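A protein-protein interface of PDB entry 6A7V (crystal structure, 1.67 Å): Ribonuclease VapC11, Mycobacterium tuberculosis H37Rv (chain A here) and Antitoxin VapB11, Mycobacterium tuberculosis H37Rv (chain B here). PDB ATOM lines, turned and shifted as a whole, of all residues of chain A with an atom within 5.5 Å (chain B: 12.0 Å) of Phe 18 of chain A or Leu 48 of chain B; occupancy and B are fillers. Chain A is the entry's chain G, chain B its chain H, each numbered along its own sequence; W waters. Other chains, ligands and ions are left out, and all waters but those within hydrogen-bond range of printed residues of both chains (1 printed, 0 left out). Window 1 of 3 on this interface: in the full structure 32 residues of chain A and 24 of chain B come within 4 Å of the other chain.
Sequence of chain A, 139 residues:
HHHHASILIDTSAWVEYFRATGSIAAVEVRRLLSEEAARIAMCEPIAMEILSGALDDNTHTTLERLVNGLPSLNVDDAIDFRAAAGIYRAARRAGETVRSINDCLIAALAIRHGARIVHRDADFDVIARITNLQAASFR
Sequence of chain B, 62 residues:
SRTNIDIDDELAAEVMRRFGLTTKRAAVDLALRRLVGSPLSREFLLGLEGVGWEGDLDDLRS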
ATOM      1  N   ALA A  13     -17.747   0.247   4.999  1.00  0.00           N
ATOM      2  CA  ALA A  13     -18.090  -1.141   5.098  1.00  0.00           C
ATOM      3  C   ALA A  13     -17.850  -1.933   3.782  1.00  0.00           C
ATOM      4  O   ALA A  13     -17.282  -3.001   3.798  1.00  0.00           O
ATOM      5  CB  ALA A  13     -19.542  -1.293   5.540  1.00  0.00           C
ATOM      6  N   TRP A  14     -18.144  -1.245   2.681  1.00  0.00           N
ATOM      7  CA  TRP A  14     -17.977  -1.785   1.359  1.00  0.00           C
ATOM      8  C   TRP A  14     -16.523  -2.213   1.143  1.00  0.00           C
ATOM      9  O   TRP A  14     -16.283  -3.258   0.551  1.00  0.00           O
ATOM     10  CB  TRP A  14     -18.390  -0.836   0.237  1.00  0.00           C
ATOM     11  CG  TRP A  14     -19.835  -0.909  -0.156  1.00  0.00           C
ATOM     12  CD1 TRP A  14     -20.729   0.099  -0.088  1.00  0.00           C
ATOM     13  CD2 TRP A  14     -20.548  -2.045  -0.683  1.00  0.00           C
ATOM     14  NE1 TRP A  14     -21.954  -0.318  -0.542  1.00  0.00           N
ATOM     15  CE2 TRP A  14     -21.873  -1.630  -0.912  1.00  0.00           C
ATOM     16  CE3 TRP A  14     -20.194  -3.363  -0.984  1.00  0.00           C
ATOM     17  CZ2 TRP A  14     -22.859  -2.488  -1.422  1.00  0.00           C
ATOM     18  CZ3 TRP A  14     -21.168  -4.216  -1.492  1.00  0.00           C
ATOM     19  CH2 TRP A  14     -22.483  -3.774  -1.707  1.00  0.00           C
ATOM     20  N   VAL A  15     -15.594  -1.296   1.441  1.00  0.00           N
ATOM     21  CA  VAL A  15     -14.203  -1.523   1.223  1.00  0.00           C
ATOM     22  C   VAL A  15     -13.731  -2.801   1.921  1.00  0.00           C
ATOM     23  O   VAL A  15     -12.968  -3.563   1.290  1.00  0.00           O
ATOM     24  CB  VAL A  15     -13.353  -0.302   1.648  1.00  0.00           C
ATOM     25  CG1 VAL A  15     -11.869  -0.648   1.701  1.00  0.00           C
ATOM     26  CG2 VAL A  15     -13.584   0.849   0.678  1.00  0.00           C
ATOM     27  N   GLU A  16     -14.155  -3.018   3.172  1.00  0.00           N
ATOM     28  CA  GLU A  16     -13.782  -4.193   3.884  1.00  0.00           C
ATOM     29  C   GLU A  16     -14.176  -5.471   3.137  1.00  0.00           C
ATOM     30  O   GLU A  16     -13.454  -6.433   3.034  1.00  0.00           O
ATOM     31  CB  GLU A  16     -14.443  -4.223   5.268  1.00  0.00           C
ATOM     32  CG  GLU A  16     -14.031  -3.087   6.191  1.00  0.00           C
ATOM     33  CD  GLU A  16     -12.571  -3.160   6.581  1.00  0.00           C
ATOM     34  OE1 GLU A  16     -12.131  -4.241   7.024  1.00  0.00           O
ATOM     35  OE2 GLU A  16     -11.872  -2.134   6.449  1.00  0.00           O
ATOM     36  N   TYR A  17     -15.431  -5.442   2.679  1.00  0.00           N
ATOM     37  CA  TYR A  17     -16.031  -6.536   1.914  1.00  0.00           C
ATOM     38  C   TYR A  17     -15.217  -6.825   0.633  1.00  0.00           C
ATOM     39  O   TYR A  17     -14.867  -7.981   0.353  1.00  0.00           O
ATOM     40  CB  TYR A  17     -17.482  -6.192   1.563  1.00  0.00           C
ATOM     41  CG  TYR A  17     -18.230  -7.317   0.886  1.00  0.00           C
ATOM     42  CD1 TYR A  17     -18.544  -8.482   1.568  1.00  0.00           C
ATOM     43  CD2 TYR A  17     -18.614  -7.206  -0.448  1.00  0.00           C
ATOM     44  CE1 TYR A  17     -19.231  -9.518   0.951  1.00  0.00           C
ATOM     45  CE2 TYR A  17     -19.298  -8.229  -1.076  1.00  0.00           C
ATOM     46  CZ  TYR A  17     -19.600  -9.378  -0.379  1.00  0.00           C
ATOM     47  OH  TYR A  17     -20.281 -10.386  -1.015  1.00  0.00           O
ATOM     48  N   PHE A  18     -14.866  -5.739  -0.034  1.00  0.00           N
ATOM     49  CA  PHE A  18     -14.098  -5.788  -1.266  1.00  0.00           C
ATOM     50  C   PHE A  18     -12.745  -6.446  -1.034  1.00  0.00           C
ATOM     51  O   PHE A  18     -12.333  -7.309  -1.818  1.00  0.00           O
ATOM     52  CB  PHE A  18     -13.948  -4.415  -1.932  1.00  0.00           C
ATOM     53  CG  PHE A  18     -15.243  -3.831  -2.442  1.00  0.00           C
ATOM     54  CD1 PHE A  18     -16.271  -4.644  -2.919  1.00  0.00           C
ATOM     55  CD2 PHE A  18     -15.427  -2.454  -2.462  1.00  0.00           C
ATOM     56  CE1 PHE A  18     -17.451  -4.095  -3.379  1.00  0.00           C
ATOM     57  CE2 PHE A  18     -16.604  -1.901  -2.929  1.00  0.00           C
ATOM     58  CZ  PHE A  18     -17.622  -2.720  -3.386  1.00  0.00           C
ATOM     59  N   ARG A  19     -12.102  -6.065   0.097  1.00  0.00           N
ATOM     60  CA  ARG A  19     -10.783  -6.557   0.404  1.00  0.00           C
ATOM     61  C   ARG A  19     -10.739  -7.962   1.028  1.00  0.00           C
ATOM     62  O   ARG A  19      -9.690  -8.519   1.177  1.00  0.00           O
ATOM     63  CB  ARG A  19     -10.054  -5.546   1.289  1.00  0.00           C
ATOM     64  CG  ARG A  19      -9.677  -4.284   0.532  1.00  0.00           C
ATOM     65  CD  ARG A  19      -9.148  -3.209   1.457  1.00  0.00           C
ATOM     66  NE  ARG A  19      -8.677  -2.046   0.709  1.00  0.00           N
ATOM     67  CZ  ARG A  19      -8.296  -0.895   1.259  1.00  0.00           C
ATOM     68  NH1 ARG A  19      -8.325  -0.732   2.579  1.00  0.00           N
ATOM     69  NH2 ARG A  19      -7.884   0.103   0.485  1.00  0.00           N
ATOM     70  N   ALA A  20     -11.911  -8.475   1.402  1.00  0.00           N
ATOM     71  CA  ALA A  20     -12.041  -9.734   2.124  1.00  0.00           C
ATOM     72  C   ALA A  20     -11.211  -9.702   3.404  1.00  0.00           C
ATOM     73  O   ALA A  20     -10.471 -10.632   3.692  1.00  0.00           O
ATOM     74  CB  ALA A  20     -11.648 -10.912   1.239  1.00  0.00           C
ATOM     75  N   ILE A  50     -16.387   4.869  -4.378  1.00  0.00           N
ATOM     76  CA  ILE A  50     -16.084   3.470  -4.667  1.00  0.00           C
ATOM     77  C   ILE A  50     -15.302   3.390  -5.985  1.00  0.00           C
ATOM     78  O   ILE A  50     -14.261   2.695  -6.094  1.00  0.00           O
ATOM     79  CB  ILE A  50     -17.358   2.588  -4.735  1.00  0.00           C
ATOM     80  CG1 ILE A  50     -17.872   2.304  -3.320  1.00  0.00           C
ATOM     81  CG2 ILE A  50     -17.074   1.273  -5.455  1.00  0.00           C
ATOM     82  CD1 ILE A  50     -19.207   1.588  -3.271  1.00  0.00           C
ATOM     83  N   THR A  62     -16.224  -3.949 -12.898  1.00  0.00           N
ATOM     84  CA  THR A  62     -17.007  -4.800 -12.026  1.00  0.00           C
ATOM     85  C   THR A  62     -17.831  -3.932 -11.031  1.00  0.00           C
ATOM     86  O   THR A  62     -19.025  -4.162 -10.838  1.00  0.00           O
ATOM     87  CB  THR A  62     -16.145  -5.843 -11.284  1.00  0.00           C
ATOM     88  OG1 THR A  62     -15.531  -6.715 -12.238  1.00  0.00           O
ATOM     89  CG2 THR A  62     -16.995  -6.682 -10.336  1.00  0.00           C
ATOM     90  N   LEU A  63     -17.147  -2.941 -10.453  1.00  0.00           N
ATOM     91  CA  LEU A  63     -17.749  -2.118  -9.452  1.00  0.00           C
ATOM     92  C   LEU A  63     -18.802  -1.189 -10.024  1.00  0.00           C
ATOM     93  O   LEU A  63     -19.812  -0.909  -9.413  1.00  0.00           O
ATOM     94  CB  LEU A  63     -16.695  -1.377  -8.621  1.00  0.00           C
ATOM     95  CG  LEU A  63     -15.851  -2.300  -7.724  1.00  0.00           C
ATOM     96  CD1 LEU A  63     -14.844  -1.496  -6.917  1.00  0.00           C
ATOM     97  CD2 LEU A  63     -16.711  -3.150  -6.793  1.00  0.00           C
ATOM     98  N   LEU A  66     -22.006  -3.075 -10.124  1.00  0.00           N
ATOM     99  CA  LEU A  66     -22.594  -3.059  -8.815  1.00  0.00           C
ATOM    100  C   LEU A  66     -23.353  -1.708  -8.563  1.00  0.00           C
ATOM    101  O   LEU A  66     -24.521  -1.667  -8.154  1.00  0.00           O
ATOM    102  CB  LEU A  66     -21.543  -3.261  -7.715  1.00  0.00           C
ATOM    103  CG  LEU A  66     -22.026  -3.003  -6.279  1.00  0.00           C
ATOM    104  CD1 LEU A  66     -23.042  -4.056  -5.853  1.00  0.00           C
ATOM    105  CD2 LEU A  66     -20.867  -2.954  -5.299  1.00  0.00           C
ATOM    106  N   SER B  38     -30.962  -2.938 -11.383  1.00  0.00           N
ATOM    107  CA  SER B  38     -30.889  -3.886 -12.479  1.00  0.00           C
ATOM    108  C   SER B  38     -30.649  -5.253 -11.862  1.00  0.00           C
ATOM    109  O   SER B  38     -30.188  -5.335 -10.720  1.00  0.00           O
ATOM    110  CB  SER B  38     -29.737  -3.529 -13.422  1.00  0.00           C
ATOM    111  OG  SER B  38     -29.800  -2.173 -13.828  1.00  0.00           O
ATOM    112  N   PRO B  39     -30.966  -6.332 -12.602  1.00  0.00           N
ATOM    113  CA  PRO B  39     -30.715  -7.674 -12.077  1.00  0.00           C
ATOM    114  C   PRO B  39     -29.270  -7.863 -11.610  1.00  0.00           C
ATOM    115  O   PRO B  39     -28.346  -7.882 -12.427  1.00  0.00           O
ATOM    116  CB  PRO B  39     -31.032  -8.587 -13.272  1.00  0.00           C
ATOM    117  CG  PRO B  39     -32.000  -7.812 -14.095  1.00  0.00           C
ATOM    118  CD  PRO B  39     -31.620  -6.369 -13.925  1.00  0.00           C
ATOM    119  N   LEU B  40     -29.087  -7.956 -10.295  1.00  0.00           N
ATOM    120  CA  LEU B  40     -27.810  -8.340  -9.709  1.00  0.00           C
ATOM    121  C   LEU B  40     -27.993  -9.694  -9.050  1.00  0.00           C
ATOM    122  O   LEU B  40     -28.623  -9.798  -7.993  1.00  0.00           O
ATOM    123  CB  LEU B  40     -27.337  -7.311  -8.678  1.00  0.00           C
ATOM    124  CG  LEU B  40     -26.875  -5.944  -9.199  1.00  0.00           C
ATOM    125  CD1 LEU B  40     -26.304  -5.133  -8.047  1.00  0.00           C
ATOM    126  CD2 LEU B  40     -25.848  -6.077 -10.315  1.00  0.00           C
ATOM    127  N   SER B  41     -27.455 -10.731  -9.687  1.00  0.00           N
ATOM    128  CA  SER B  41     -27.603 -12.093  -9.189  1.00  0.00           C
ATOM    129  C   SER B  41     -26.877 -12.262  -7.863  1.00  0.00           C
ATOM    130  O   SER B  41     -25.965 -11.498  -7.530  1.00  0.00           O
ATOM    131  CB  SER B  41     -27.081 -13.112 -10.208  1.00  0.00           C
ATOM    132  OG  SER B  41     -25.683 -12.988 -10.397  1.00  0.00           O
ATOM    133  N   ARG B  42     -27.297 -13.276  -7.117  1.00  0.00           N
ATOM    134  CA  ARG B  42     -26.741 -13.558  -5.801  1.00  0.00           C
ATOM    135  C   ARG B  42     -25.259 -13.910  -5.938  1.00  0.00           C
ATOM    136  O   ARG B  42     -24.442 -13.489  -5.129  1.00  0.00           O
ATOM    137  CB  ARG B  42     -27.492 -14.727  -5.152  1.00  0.00           C
ATOM    138  CG  ARG B  42     -26.967 -15.156  -3.790  1.00  0.00           C
ATOM    139  CD  ARG B  42     -27.550 -16.500  -3.382  1.00  0.00           C
ATOM    140  NE  ARG B  42     -27.189 -16.867  -2.016  1.00  0.00           N
ATOM    141  CZ  ARG B  42     -27.758 -16.370  -0.919  1.00  0.00           C
ATOM    142  NH1 ARG B  42     -28.733 -15.467  -1.000  1.00  0.00           N
ATOM    143  NH2 ARG B  42     -27.348 -16.780   0.276  1.00  0.00           N
ATOM    144  N   GLU B  43     -24.926 -14.685  -6.964  1.00  0.00           N
ATOM    145  CA  GLU B  43     -23.541 -15.106  -7.136  1.00  0.00           C
ATOM    146  C   GLU B  43     -22.663 -13.897  -7.431  1.00  0.00           C
ATOM    147  O   GLU B  43     -21.559 -13.781  -6.886  1.00  0.00           O
ATOM    148  CB  GLU B  43     -23.401 -16.154  -8.249  1.00  0.00           C
ATOM    149  CG  GLU B  43     -21.968 -16.627  -8.486  1.00  0.00           C
ATOM    150  CD  GLU B  43     -21.229 -16.955  -7.197  1.00  0.00           C
ATOM    151  OE1 GLU B  43     -21.623 -17.932  -6.520  1.00  0.00           O
ATOM    152  OE2 GLU B  43     -20.262 -16.232  -6.859  1.00  0.00           O
ATOM    153  N   PHE B  44     -23.143 -12.995  -8.274  1.00  0.00           N
ATOM    154  CA  PHE B  44     -22.379 -11.775  -8.544  1.00  0.00           C
ATOM    155  C   PHE B  44     -22.009 -11.062  -7.226  1.00  0.00           C
ATOM    156  O   PHE B  44     -20.841 -10.720  -6.991  1.00  0.00           O
ATOM    157  CB  PHE B  44     -23.167 -10.831  -9.458  1.00  0.00           C
ATOM    158  CG  PHE B  44     -22.505  -9.496  -9.666  1.00  0.00           C
ATOM    159  CD1 PHE B  44     -21.425  -9.370 -10.528  1.00  0.00           C
ATOM    160  CD2 PHE B  44     -22.963  -8.366  -8.998  1.00  0.00           C
ATOM    161  CE1 PHE B  44     -20.811  -8.143 -10.720  1.00  0.00           C
ATOM    162  CE2 PHE B  44     -22.352  -7.138  -9.188  1.00  0.00           C
ATOM    163  CZ  PHE B  44     -21.276  -7.025 -10.049  1.00  0.00           C
ATOM    164  N   LEU B  45     -23.034 -10.748  -6.443  1.00  0.00           N
ATOM    165  CA  LEU B  45     -22.859 -10.015  -5.214  1.00  0.00           C
ATOM    166  C   LEU B  45     -21.931 -10.786  -4.250  1.00  0.00           C
ATOM    167  O   LEU B  45     -21.041 -10.161  -3.648  1.00  0.00           O
ATOM    168  CB  LEU B  45     -24.211  -9.744  -4.543  1.00  0.00           C
ATOM    169  CG  LEU B  45     -25.173  -8.800  -5.273  1.00  0.00           C
ATOM    170  CD1 LEU B  45     -26.556  -8.843  -4.635  1.00  0.00           C
ATOM    171  CD2 LEU B  45     -24.637  -7.374  -5.285  1.00  0.00           C
ATOM    172  N   LEU B  46     -22.090 -12.099  -4.143  1.00  0.00           N
ATOM    173  CA  LEU B  46     -21.206 -12.808  -3.249  1.00  0.00           C
ATOM    174  C   LEU B  46     -19.772 -12.840  -3.753  1.00  0.00           C
ATOM    175  O   LEU B  46     -18.862 -12.686  -2.978  1.00  0.00           O
ATOM    176  CB  LEU B  46     -21.729 -14.218  -2.964  1.00  0.00           C
ATOM    177  CG  LEU B  46     -23.021 -14.269  -2.140  1.00  0.00           C
ATOM    178  CD1 LEU B  46     -23.390 -15.713  -1.839  1.00  0.00           C
ATOM    179  CD2 LEU B  46     -22.912 -13.471  -0.846  1.00  0.00           C
ATOM    180  N   GLY B  47     -19.603 -12.901  -5.056  1.00  0.00           N
ATOM    181  CA  GLY B  47     -18.329 -12.914  -5.731  1.00  0.00           C
ATOM    182  C   GLY B  47     -17.512 -11.646  -5.618  1.00  0.00           C
ATOM    183  O   GLY B  47     -16.340 -11.656  -5.943  1.00  0.00           O
ATOM    184  N   LEU B  48     -18.146 -10.551  -5.198  1.00  0.00           N
ATOM    185  CA  LEU B  48     -17.449  -9.285  -4.992  1.00  0.00           C
ATOM    186  C   LEU B  48     -16.579  -9.298  -3.743  1.00  0.00           C
ATOM    187  O   LEU B  48     -15.678  -8.468  -3.612  1.00  0.00           O
ATOM    188  CB  LEU B  48     -18.448  -8.130  -4.905  1.00  0.00           C
ATOM    189  CG  LEU B  48     -19.266  -7.860  -6.169  1.00  0.00           C
ATOM    190  CD1 LEU B  48     -20.353  -6.838  -5.879  1.00  0.00           C
ATOM    191  CD2 LEU B  48     -18.374  -7.401  -7.310  1.00  0.00           C
ATOM    192  N   GLU B  49     -16.844 -10.220  -2.820  1.00  0.00           N
ATOM    193  CA  GLU B  49     -15.991 -10.361  -1.649  1.00  0.00           C
ATOM    194  C   GLU B  49     -14.604 -10.828  -2.090  1.00  0.00           C
ATOM    195  O   GLU B  49     -14.454 -11.926  -2.619  1.00  0.00           O
ATOM    196  CB  GLU B  49     -16.587 -11.335  -0.635  1.00  0.00           C
ATOM    197  CG  GLU B  49     -15.908 -11.265   0.724  1.00  0.00           C
ATOM    198  CD  GLU B  49     -16.736 -11.865   1.842  1.00  0.00           C
ATOM    199  OE1 GLU B  49     -16.473 -11.516   3.013  1.00  0.00           O
ATOM    200  OE2 GLU B  49     -17.645 -12.679   1.564  1.00  0.00           O
ATOM    201  N   GLY B  50     -13.604  -9.973  -1.890  1.00  0.00           N
ATOM    202  CA  GLY B  50     -12.233 -10.266  -2.303  1.00  0.00           C
ATOM    203  C   GLY B  50     -11.873  -9.769  -3.693  1.00  0.00           C
ATOM    204  O   GLY B  50     -10.785 -10.060  -4.186  1.00  0.00           O
ATOM    205  N   VAL B  51     -12.768  -9.012  -4.330  1.00  0.00           N
ATOM    206  CA  VAL B  51     -12.492  -8.477  -5.668  1.00  0.00           C
ATOM    207  C   VAL B  51     -11.347  -7.462  -5.632  1.00  0.00           C
ATOM    208  O   VAL B  51     -10.667  -7.255  -6.637  1.00  0.00           O
ATOM    209  CB  VAL B  51     -13.746  -7.846  -6.320  1.00  0.00           C
ATOM    210  CG1 VAL B  51     -14.087  -6.500  -5.686  1.00  0.00           C
ATOM    211  CG2 VAL B  51     -13.552  -7.699  -7.825  1.00  0.00           C
ATOM    212  N   GLY B  52     -11.141  -6.839  -4.473  1.00  0.00           N
ATOM    213  CA  GLY B  52     -10.032  -5.916  -4.267  1.00  0.00           C
ATOM    214  C   GLY B  52     -10.449  -4.461  -4.388  1.00  0.00           C
ATOM    215  O   GLY B  52     -11.339  -4.119  -5.171  1.00  0.00           O
ATOM    216  N   TRP B  53      -9.805  -3.608  -3.598  1.00  0.00           N
ATOM    217  CA  TRP B  53     -10.009  -2.164  -3.669  1.00  0.00           C
ATOM    218  C   TRP B  53      -8.714  -1.499  -3.225  1.00  0.00           C
ATOM    219  O   TRP B  53      -8.449  -1.381  -2.029  1.00  0.00           O
ATOM    220  CB  TRP B  53     -11.185  -1.748  -2.782  1.00  0.00           C
ATOM    221  CG  TRP B  53     -11.729  -0.381  -3.074  1.00  0.00           C
ATOM    222  CD1 TRP B  53     -12.591  -0.041  -4.072  1.00  0.00           C
ATOM    223  CD2 TRP B  53     -11.459   0.825  -2.350  1.00  0.00           C
ATOM    224  NE1 TRP B  53     -12.869   1.304  -4.021  1.00  0.00           N
ATOM    225  CE2 TRP B  53     -12.192   1.857  -2.968  1.00  0.00           C
ATOM    226  CE3 TRP B  53     -10.673   1.131  -1.233  1.00  0.00           C
ATOM    227  CZ2 TRP B  53     -12.163   3.179  -2.508  1.00  0.00           C
ATOM    228  CZ3 TRP B  53     -10.641   2.443  -0.778  1.00  0.00           C
ATOM    229  CH2 TRP B  53     -11.379   3.452  -1.419  1.00  0.00           C
ATOM    230  N   GLU B  54      -7.906  -1.087  -4.197  1.00  0.00           N
ATOM    231  CA  GLU B  54      -6.529  -0.660  -3.935  1.00  0.00           C
ATOM    232  C   GLU B  54      -6.394   0.825  -3.618  1.00  0.00           C
ATOM    233  O   GLU B  54      -5.317   1.279  -3.247  1.00  0.00           O
ATOM    234  CB  GLU B  54      -5.632  -1.025  -5.119  1.00  0.00           C
ATOM    235  CG  GLU B  54      -5.507  -2.524  -5.337  1.00  0.00           C
ATOM    236  CD  GLU B  54      -4.449  -2.884  -6.360  1.00  0.00           C
ATOM    237  OE1 GLU B  54      -3.512  -3.627  -6.004  1.00  0.00           O
ATOM    238  OE2 GLU B  54      -4.549  -2.421  -7.517  1.00  0.00           O
ATOM    239  N   GLY B  55      -7.483   1.577  -3.754  1.00  0.00           N
ATOM    240  CA  GLY B  55      -7.481   2.990  -3.396  1.00  0.00           C
ATOM    241  C   GLY B  55      -7.304   3.194  -1.907  1.00  0.00           C
ATOM    242  O   GLY B  55      -7.243   2.233  -1.136  1.00  0.00           O
ATOM    243  N   ASP B  56      -7.214   4.457  -1.509  1.00  0.00           N
ATOM    244  CA  ASP B  56      -7.047   4.823  -0.112  1.00  0.00           C
ATOM    245  C   ASP B  56      -8.260   5.649   0.305  1.00  0.00           C
ATOM    246  O   ASP B  56      -8.432   6.773  -0.162  1.00  0.00           O
ATOM    247  CB  ASP B  56      -5.750   5.625   0.064  1.00  0.00           C
ATOM    248  CG  ASP B  56      -5.322   5.756   1.520  1.00  0.00           C
ATOM    249  OD1 ASP B  56      -6.141   5.497   2.425  1.00  0.00           O
ATOM    250  OD2 ASP B  56      -4.154   6.125   1.761  1.00  0.00           O
ATOM    251  N   LEU B  57      -9.100   5.088   1.172  1.00  0.00           N
ATOM    252  CA  LEU B  57     -10.298   5.790   1.644  1.00  0.00           C
ATOM    253  C   LEU B  57      -9.950   7.023   2.493  1.00  0.00           C
ATOM    254  O   LEU B  57     -10.734   7.973   2.559  1.00  0.00           O
ATOM    255  CB  LEU B  57     -11.210   4.839   2.430  1.00  0.00           C
ATOM    256  CG  LEU B  57     -12.596   5.368   2.811  1.00  0.00           C
ATOM    257  CD1 LEU B  57     -13.385   5.802   1.582  1.00  0.00           C
ATOM    258  CD2 LEU B  57     -13.365   4.318   3.595  1.00  0.00           C
ATOM    259  N   LEU B  60      -9.753  10.030   0.180  1.00  0.00           N
ATOM    260  CA  LEU B  60     -11.080  10.502  -0.214  1.00  0.00           C
ATOM    261  C   LEU B  60     -11.790  11.231   0.923  1.00  0.00           C
ATOM    262  O   LEU B  60     -12.565  12.150   0.685  1.00  0.00           O
ATOM    263  CB  LEU B  60     -11.942   9.329  -0.692  1.00  0.00           C
ATOM    264  CG  LEU B  60     -11.432   8.565  -1.917  1.00  0.00           C
ATOM    265  CD1 LEU B  60     -12.305   7.345  -2.173  1.00  0.00           C
ATOM    266  CD2 LEU B  60     -11.380   9.462  -3.146  1.00  0.00           C
ATOM    267  N   ARG B  61     -11.516  10.806   2.155  1.00  0.00           N
ATOM    268  CA  ARG B  61     -12.136  11.371   3.353  1.00  0.00           C
ATOM    269  C   ARG B  61     -11.085  12.126   4.180  1.00  0.00           C
ATOM    270  O   ARG B  61     -10.946  13.336   4.019  1.00  0.00           O
ATOM    271  CB  ARG B  61     -12.831  10.247   4.142  1.00  0.00           C
ATOM    272  CG  ARG B  61     -13.956   9.607   3.340  1.00  0.00           C
ATOM    273  CD  ARG B  61     -14.797   8.622   4.138  1.00  0.00           C
ATOM    274  NE  ARG B  61     -15.971   8.205   3.372  1.00  0.00           N
ATOM    275  CZ  ARG B  61     -16.938   7.403   3.817  1.00  0.00           C
ATOM    276  NH1 ARG B  61     -16.900   6.900   5.049  1.00  0.00           N
ATOM    277  NH2 ARG B  61     -17.960   7.107   3.019  1.00  0.00           N
HETATM  278  O   HOH W   1      -8.773   2.444   2.480  1.00  0.00           O
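OG of Ser 41 of chain B is in hydrogen-bond range of N of Phe 44 of chain B, at 3.3 Å.
Of chain B, only Leu 48 (3.9 Å), Gly 50 (3.0 Å), Val 51 (3.1 Å), Gly 52 (2.9 Å) and Trp 53 (3.9 Å) come within 4 Å of Phe 18 of chain A.
Leu 48 of chain B touches four residues of chain A.
No residue of chain B comes within 4 Å of Trp 14 of chain A.
Val 15 of chain A touches one residue of chain B.
Tyr 17 of chain A touches just these residues of chain B: Leu 45, Leu 46, Leu 48, Glu 49 and Gly 50.
Ala 20 of chain A touches just one residue of chain B: Gly 50 (3.6 Å).
Of the printed residues of chain B, Ile 50 of chain A touches Trp 53 (2.9 Å).
Thr 62 of chain A touches just these residues of chain B: Phe 44 and Leu 48.
Of chain B, only Trp 53 comes within 4 Å of Leu 63 of chain A.
Printed residues of chain B within 4 Å of Leu 66 of chain A: Leu 40 (3.9 Å), Leu 45 (3.7 Å) and Leu 48 (3.9 Å).
Of the printed residues of chain A, Leu 40 of chain B touches Leu 66.
Of the printed residues of chain A, Val 51 of chain B touches Phe 18 (3.1 Å).
Of the printed residues of chain A, Gly 55 of chain B touches Arg 19 (2.8 Å).
Of the printed residues of chain A, Leu 46 of chain B touches Tyr 17.
The nearest residue of chain B that does not touch Phe 18 of chain A is Glu 49 of chain B (4.2 Å).
CG2 of Val 15 of chain A touches CE3 of Trp 53 of chain B, at 3.5 Å.
Tyr 17 of chain A touches Leu 48 of chain B.
Phe 18 of chain A touches Leu 48 of chain B (CA to O, 3.9 Å).
Trp 53 of chain B touches Phe 18 of chain A.
Ala 20 of chain A touches Gly 50 of chain B (CB to CA, 3.6 Å).
CD2 of Leu 48 of chain B touches CG2 of Thr 62 of chain A (3.4 Å).
CD1 of Leu 63 of chain A touches CD1 of Trp 53 of chain B (3.9 Å).
Leu 40 of chain B touches Leu 66 of chain A.
Leu 66 of chain A touches Leu 45 of chain B (CD1 to CD2, 3.7 Å).
CD1 of Leu 66 of chain A touches CD1 of Leu 48 of chain B, 3.9 Å away.
Water W1 bridges the backbone NH of Leu 57 of chain B and the guanidinium group of Arg 19 of chain A.
Of the 12 printed residues of chain A, 9 touch a printed residue of chain B.
Printed residues of chain A that touch a printed residue of chain B: Val 15, Tyr 17, Phe 18, Arg 19, Ala 20, Ile 50, Thr 62, Leu 63 and Leu 66.
Along chain A the printed residues that touch a printed residue of chain B span positions 15 to 66.
Among the printed residues, no Asp or Glu carboxylate lies within 4 Å of a Lys or Arg side-chain nitrogen of the other chain.
The indole nitrogen (NE1) of Trp 53 of chain B is in hydrogen-bond range of the backbone carbonyl oxygen (O) of Ile 50 of chain A (2.9 Å).
The backbone carbonyl oxygen (O) of Leu 46 of chain B sits at hydrogen-bond distance from the side-chain hydroxyl (OH) of Tyr 17 of chain A (3.3 Å).
The backbone carbonyl oxygen (O) of Phe 18 of chain A lies within hydrogen-bond range of the backbone NH (N) of Val 51 of chain B.
O of Tyr 17 of chain A lies within hydrogen-bond range of N of Gly 50 of chain B, 3.3 Å away.
N of Gly 50 of chain B is in hydrogen-bond range of O of Phe 18 of chain A (3.0 Å).
The backbone carbonyl oxygen of Trp 53 of chain B is in hydrogen-bond range of the guanidinium group of Arg 19 of chain A (2.8 Å).
The side-chain hydroxyl (OH) of Tyr 17 of chain A is in hydrogen-bond range of the backbone carbonyl oxygen (O) of Leu 45 of chain B, 2.7 Å away.
O of Phe 18 of chain A is in hydrogen-bond range of N of Gly 52 of chain B, 2.9 Å away.
The guanidinium group (NH2) of Arg 19 of chain A lies within hydrogen-bond range of the backbone carbonyl oxygen (O) of Gly 55 of chain B (2.8 Å).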
